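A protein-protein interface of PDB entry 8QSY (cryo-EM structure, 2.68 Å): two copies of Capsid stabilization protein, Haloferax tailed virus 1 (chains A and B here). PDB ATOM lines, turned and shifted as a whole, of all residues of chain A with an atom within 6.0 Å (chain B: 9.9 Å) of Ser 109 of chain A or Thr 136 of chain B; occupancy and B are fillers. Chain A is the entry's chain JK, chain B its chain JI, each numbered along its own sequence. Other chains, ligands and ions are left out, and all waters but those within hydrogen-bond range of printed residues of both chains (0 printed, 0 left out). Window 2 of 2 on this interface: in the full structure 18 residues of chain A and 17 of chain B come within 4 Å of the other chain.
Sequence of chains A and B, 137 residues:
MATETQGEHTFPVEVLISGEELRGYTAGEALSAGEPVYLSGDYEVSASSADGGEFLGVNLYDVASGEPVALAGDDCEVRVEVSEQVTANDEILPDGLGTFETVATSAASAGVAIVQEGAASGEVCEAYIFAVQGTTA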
ATOM      1  N   ASN A  89       8.085  -1.629  -0.151  1.00  0.00           N
ATOM      2  CA  ASN A  89       8.296  -1.478  -1.584  1.00  0.00           C
ATOM      3  C   ASN A  89       7.088  -0.913  -2.351  1.00  0.00           C
ATOM      4  O   ASN A  89       7.233  -0.677  -3.550  1.00  0.00           O
ATOM      5  CB  ASN A  89       8.843  -2.749  -2.250  1.00  0.00           C
ATOM      6  CG  ASN A  89       9.691  -2.482  -3.477  1.00  0.00           C
ATOM      7  OD1 ASN A  89      10.740  -1.851  -3.385  1.00  0.00           O
ATOM      8  ND2 ASN A  89       9.266  -2.975  -4.631  1.00  0.00           N
ATOM      9  N   GLU A  91       5.100   1.948  -3.968  1.00  0.00           N
ATOM     10  CA  GLU A  91       5.119   3.382  -4.208  1.00  0.00           C
ATOM     11  C   GLU A  91       3.767   3.981  -3.835  1.00  0.00           C
ATOM     12  O   GLU A  91       2.702   3.448  -4.166  1.00  0.00           O
ATOM     13  CB  GLU A  91       5.490   3.718  -5.646  1.00  0.00           C
ATOM     14  CG  GLU A  91       6.949   3.457  -5.935  1.00  0.00           C
ATOM     15  CD  GLU A  91       7.478   4.028  -7.243  1.00  0.00           C
ATOM     16  OE1 GLU A  91       6.782   4.871  -7.860  1.00  0.00           O
ATOM     17  OE2 GLU A  91       8.599   3.644  -7.641  1.00  0.00           O
ATOM     18  N   VAL A 103       0.309   4.118  -5.609  1.00  0.00           N
ATOM     19  CA  VAL A 103       0.300   4.370  -7.041  1.00  0.00           C
ATOM     20  C   VAL A 103      -0.634   3.387  -7.737  1.00  0.00           C
ATOM     21  O   VAL A 103      -1.439   3.804  -8.560  1.00  0.00           O
ATOM     22  CB  VAL A 103       1.725   4.304  -7.610  1.00  0.00           C
ATOM     23  CG1 VAL A 103       1.761   4.361  -9.129  1.00  0.00           C
ATOM     24  CG2 VAL A 103       2.554   5.426  -7.035  1.00  0.00           C
ATOM     25  N   ALA A 104      -0.576   2.109  -7.353  1.00  0.00           N
ATOM     26  CA  ALA A 104      -1.434   1.063  -7.896  1.00  0.00           C
ATOM     27  C   ALA A 104      -2.929   1.389  -7.771  1.00  0.00           C
ATOM     28  O   ALA A 104      -3.702   1.030  -8.659  1.00  0.00           O
ATOM     29  CB  ALA A 104      -1.101  -0.239  -7.222  1.00  0.00           C
ATOM     30  N   THR A 105      -3.347   2.058  -6.684  1.00  0.00           N
ATOM     31  CA  THR A 105      -4.734   2.470  -6.499  1.00  0.00           C
ATOM     32  C   THR A 105      -5.066   3.739  -7.283  1.00  0.00           C
ATOM     33  O   THR A 105      -6.186   3.883  -7.780  1.00  0.00           O
ATOM     34  CB  THR A 105      -5.034   2.707  -5.016  1.00  0.00           C
ATOM     35  OG1 THR A 105      -4.774   1.467  -4.368  1.00  0.00           O
ATOM     36  CG2 THR A 105      -6.473   3.056  -4.717  1.00  0.00           C
ATOM     37  N   SER A 106      -4.108   4.670  -7.385  1.00  0.00           N
ATOM     38  CA  SER A 106      -4.287   5.958  -8.046  1.00  0.00           C
ATOM     39  C   SER A 106      -4.485   5.816  -9.561  1.00  0.00           C
ATOM     40  O   SER A 106      -4.300   4.741 -10.129  1.00  0.00           O
ATOM     41  CB  SER A 106      -3.098   6.823  -7.742  1.00  0.00           C
ATOM     42  OG  SER A 106      -1.990   6.463  -8.548  1.00  0.00           O
ATOM     43  N   ALA A 107      -4.796   6.928 -10.242  1.00  0.00           N
ATOM     44  CA  ALA A 107      -4.792   6.975 -11.701  1.00  0.00           C
ATOM     45  C   ALA A 107      -3.379   7.152 -12.282  1.00  0.00           C
ATOM     46  O   ALA A 107      -3.161   6.911 -13.473  1.00  0.00           O
ATOM     47  CB  ALA A 107      -5.736   8.054 -12.173  1.00  0.00           C
ATOM     48  N   ALA A 108      -2.415   7.582 -11.455  1.00  0.00           N
ATOM     49  CA  ALA A 108      -1.044   7.859 -11.871  1.00  0.00           C
ATOM     50  C   ALA A 108      -0.228   6.580 -12.085  1.00  0.00           C
ATOM     51  O   ALA A 108      -0.597   5.491 -11.640  1.00  0.00           O
ATOM     52  CB  ALA A 108      -0.397   8.757 -10.851  1.00  0.00           C
ATOM     53  N   SER A 109       0.943   6.743 -12.726  1.00  0.00           N
ATOM     54  CA  SER A 109       1.864   5.655 -13.051  1.00  0.00           C
ATOM     55  C   SER A 109       3.122   5.639 -12.168  1.00  0.00           C
ATOM     56  O   SER A 109       3.864   4.654 -12.183  1.00  0.00           O
ATOM     57  CB  SER A 109       2.253   5.707 -14.508  1.00  0.00           C
ATOM     58  OG  SER A 109       2.884   6.946 -14.786  1.00  0.00           O
ATOM     59  N   ALA A 110       3.386   6.724 -11.417  1.00  0.00           N
ATOM     60  CA  ALA A 110       4.621   6.889 -10.656  1.00  0.00           C
ATOM     61  C   ALA A 110       4.368   7.577  -9.311  1.00  0.00           C
ATOM     62  O   ALA A 110       3.538   8.476  -9.216  1.00  0.00           O
ATOM     63  CB  ALA A 110       5.615   7.669 -11.479  1.00  0.00           C
ATOM     64  N   GLY A 111       5.119   7.173  -8.280  1.00  0.00           N
ATOM     65  CA  GLY A 111       4.914   7.669  -6.926  1.00  0.00           C
ATOM     66  C   GLY A 111       5.884   8.780  -6.544  1.00  0.00           C
ATOM     67  O   GLY A 111       6.744   9.182  -7.323  1.00  0.00           O
ATOM     68  N   ASP B  51      15.096  -5.449 -14.625  1.00  0.00           N
ATOM     69  CA  ASP B  51      14.028  -4.733 -15.327  1.00  0.00           C
ATOM     70  C   ASP B  51      13.110  -3.884 -14.433  1.00  0.00           C
ATOM     71  O   ASP B  51      11.913  -3.740 -14.706  1.00  0.00           O
ATOM     72  CB  ASP B  51      13.298  -5.666 -16.299  1.00  0.00           C
ATOM     73  CG  ASP B  51      14.223  -6.299 -17.321  1.00  0.00           C
ATOM     74  OD1 ASP B  51      15.175  -5.607 -17.768  1.00  0.00           O
ATOM     75  OD2 ASP B  51      13.960  -7.452 -17.709  1.00  0.00           O
ATOM     76  N   GLY B  52      13.678  -3.277 -13.384  1.00  0.00           N
ATOM     77  CA  GLY B  52      13.031  -2.160 -12.703  1.00  0.00           C
ATOM     78  C   GLY B  52      12.049  -2.533 -11.588  1.00  0.00           C
ATOM     79  O   GLY B  52      11.760  -3.705 -11.335  1.00  0.00           O
ATOM     80  N   GLY B  53      11.558  -1.496 -10.894  1.00  0.00           N
ATOM     81  CA  GLY B  53      10.590  -1.636  -9.812  1.00  0.00           C
ATOM     82  C   GLY B  53      11.171  -2.181  -8.502  1.00  0.00           C
ATOM     83  O   GLY B  53      10.447  -2.311  -7.512  1.00  0.00           O
ATOM     84  N   GLU B  54      12.480  -2.482  -8.499  1.00  0.00           N
ATOM     85  CA  GLU B  54      13.163  -3.089  -7.363  1.00  0.00           C
ATOM     86  C   GLU B  54      14.541  -2.454  -7.176  1.00  0.00           C
ATOM     87  O   GLU B  54      15.561  -3.074  -7.469  1.00  0.00           O
ATOM     88  CB  GLU B  54      13.303  -4.600  -7.559  1.00  0.00           C
ATOM     89  CG  GLU B  54      12.015  -5.367  -7.355  1.00  0.00           C
ATOM     90  CD  GLU B  54      12.197  -6.875  -7.412  1.00  0.00           C
ATOM     91  OE1 GLU B  54      13.350  -7.330  -7.558  1.00  0.00           O
ATOM     92  OE2 GLU B  54      11.175  -7.593  -7.362  1.00  0.00           O
ATOM     93  N   SER B 109      12.360   1.234 -18.858  1.00  0.00           N
ATOM     94  CA  SER B 109      12.414   2.472 -19.640  1.00  0.00           C
ATOM     95  C   SER B 109      13.079   3.649 -18.905  1.00  0.00           C
ATOM     96  O   SER B 109      13.303   4.698 -19.515  1.00  0.00           O
ATOM     97  CB  SER B 109      11.046   2.853 -20.156  1.00  0.00           C
ATOM     98  OG  SER B 109      10.164   3.102 -19.072  1.00  0.00           O
ATOM     99  N   VAL B 132      15.055   6.029  -6.930  1.00  0.00           N
ATOM    100  CA  VAL B 132      14.695   4.718  -6.402  1.00  0.00           C
ATOM    101  C   VAL B 132      13.462   4.226  -7.157  1.00  0.00           C
ATOM    102  O   VAL B 132      12.724   5.032  -7.713  1.00  0.00           O
ATOM    103  CB  VAL B 132      14.499   4.724  -4.869  1.00  0.00           C
ATOM    104  CG1 VAL B 132      15.679   5.359  -4.151  1.00  0.00           C
ATOM    105  CG2 VAL B 132      13.202   5.372  -4.414  1.00  0.00           C
ATOM    106  N   GLN B 133      13.261   2.904  -7.208  1.00  0.00           N
ATOM    107  CA  GLN B 133      12.116   2.327  -7.891  1.00  0.00           C
ATOM    108  C   GLN B 133      11.448   1.293  -6.994  1.00  0.00           C
ATOM    109  O   GLN B 133      12.096   0.357  -6.524  1.00  0.00           O
ATOM    110  CB  GLN B 133      12.550   1.675  -9.203  1.00  0.00           C
ATOM    111  CG  GLN B 133      13.039   2.678 -10.236  1.00  0.00           C
ATOM    112  CD  GLN B 133      13.408   2.045 -11.554  1.00  0.00           C
ATOM    113  OE1 GLN B 133      13.274   0.839 -11.751  1.00  0.00           O
ATOM    114  NE2 GLN B 133      13.907   2.862 -12.470  1.00  0.00           N
ATOM    115  N   GLY B 134      10.131   1.449  -6.818  1.00  0.00           N
ATOM    116  CA  GLY B 134       9.315   0.510  -6.071  1.00  0.00           C
ATOM    117  C   GLY B 134       8.194  -0.085  -6.918  1.00  0.00           C
ATOM    118  O   GLY B 134       8.144   0.084  -8.137  1.00  0.00           O
ATOM    119  N   THR B 135       7.278  -0.777  -6.232  1.00  0.00           N
ATOM    120  CA  THR B 135       6.107  -1.393  -6.830  1.00  0.00           C
ATOM    121  C   THR B 135       5.100  -0.310  -7.216  1.00  0.00           C
ATOM    122  O   THR B 135       4.501   0.314  -6.344  1.00  0.00           O
ATOM    123  CB  THR B 135       5.436  -2.362  -5.845  1.00  0.00           C
ATOM    124  OG1 THR B 135       6.393  -2.904  -4.934  1.00  0.00           O
ATOM    125  CG2 THR B 135       4.694  -3.480  -6.540  1.00  0.00           C
ATOM    126  N   THR B 136       4.893  -0.117  -8.527  1.00  0.00           N
ATOM    127  CA  THR B 136       3.844   0.761  -9.040  1.00  0.00           C
ATOM    128  C   THR B 136       2.576   0.002  -9.436  1.00  0.00           C
ATOM    129  O   THR B 136       1.522   0.620  -9.602  1.00  0.00           O
ATOM    130  CB  THR B 136       4.320   1.546 -10.270  1.00  0.00           C
ATOM    131  OG1 THR B 136       4.727   0.636 -11.292  1.00  0.00           O
ATOM    132  CG2 THR B 136       5.455   2.488  -9.939  1.00  0.00           C
ATOM    133  N   ALA B 137       2.685  -1.332  -9.584  1.00  0.00           N
ATOM    134  CA  ALA B 137       1.822  -2.147 -10.442  1.00  0.00           C
ATOM    135  C   ALA B 137       1.758  -1.590 -11.884  1.00  0.00           C
ATOM    136  O   ALA B 137       0.850  -2.041 -12.635  1.00  0.00           O
ATOM    137  CB  ALA B 137       0.460  -2.371  -9.808  1.00  0.00           C
ATOM    138  OXT ALA B 137       2.643  -0.752 -12.245  1.00  0.00           O
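ND2 of Asn 89 of chain A lies within hydrogen-bond range of O of Gly 53 of chain B (3.2 Å).
N of Gly 134 of chain B is in hydrogen-bond range of OE2 of Glu 91 of chain A (2.8 Å).
The backbone carbonyl oxygen (O) of Asn 89 of chain A sits at hydrogen-bond distance from the backbone NH (N) of Thr 135 of chain B (2.7 Å).
O of Thr 135 of chain B is in hydrogen-bond range of N of Glu 91 of chain A (2.9 Å).
The backbone NH of Ala 104 of chain A lies within hydrogen-bond range of the backbone carbonyl oxygen of Thr 136 of chain B.
The backbone NH of Gly 53 of chain B sits at hydrogen-bond distance from the side-chain amide oxygen of Gln 133 of chain B (3.0 Å).
The backbone carbonyl oxygen (O) of Gln 133 of chain B is in hydrogen-bond range of the backbone NH (N) of Glu 54 of chain B, 3.5 Å away.
O of Glu 91 of chain A lies within hydrogen-bond range of N of Val 103 of chain A.
The backbone NH of Gly 111 of chain A is in hydrogen-bond range of the side-chain carboxylate of Glu 91 of chain A (2.9 Å).
The backbone carbonyl oxygen (O) of Val 103 of chain A sits at hydrogen-bond distance from the side-chain hydroxyl (OG) of Ser 106 of chain A, at 2.7 Å.
Among the printed residues, merely in contact across the chains: Glu 91 of chain A with Thr 136 of chain B, Asn 89 of chain A with Gly 134 of chain B, Ser 109 of chain A with Thr 136 of chain B, Ala 104 of chain A with Ala 137 of chain B, Glu 91 of chain A with Gln 133 of chain B and Val 103 of chain A with Thr 136 of chain B.
Of the printed residues of chain B, Asn 89 of chain A touches Gly 53 (3.2 Å), Gly 134 (3.5 Å) and Thr 135 (2.7 Å).
Printed residues of chain B within 4 Å of Glu 91 of chain A: Gln 133, Gly 134, Thr 135 and Thr 136.
Val 103 of chain A touches just one residue of chain B: Thr 136 (3.8 Å).
Ala 104 of chain A touches just these residues of chain B: Thr 136 and Ala 137.
No residue of chain B comes within 4 Å of Ala 108 of chain A.
Of chain B, only Thr 136 (3.5 Å) comes within 4 Å of Ser 109 of chain A.
No residue of chain B comes within 4 Å of Ala 110 of chain A.
Gly 111 of chain A touches none of the printed residues of chain B.
Of the printed residues of chain A, Gly 134 of chain B touches Asn 89 and Glu 91.
Of the printed residues of chain A, Thr 135 of chain B touches Asn 89 (2.7 Å) and Glu 91 (2.9 Å).
Of chain A, only Glu 91 (3.4 Å), Val 103 (3.8 Å), Ala 104 (3.4 Å) and Ser 109 (3.5 Å) come within 4 Å of Thr 136 of chain B.
The nearest residue of chain A that does not touch Thr 136 of chain B is Ala 110 of chain A (4.5 Å).
The nearest printed residue of chain A that does not touch Gly 53 of chain B is Glu 91 of chain A (6.0 Å).
Of the 11 printed residues of chain A, 5 touch a printed residue of chain B.
Hydrophobic or aromatic side chains of chain A within 4 Å of the printed part of chain B: Val 103 and Ala 104.
Of the 11 printed residues of chain B, 6 touch a printed residue of chain A.
Among the printed residues, 11 pairs touch across the chains.
Among the printed residues, no Asp or Glu carboxylate lies within 4 Å of a Lys or Arg side-chain nitrogen of the other chain.
Position printed for both chains: 109.
Of the 11 pairs that touch across the chains among the printed residues, none has its exchanged pair printed and touching as well.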
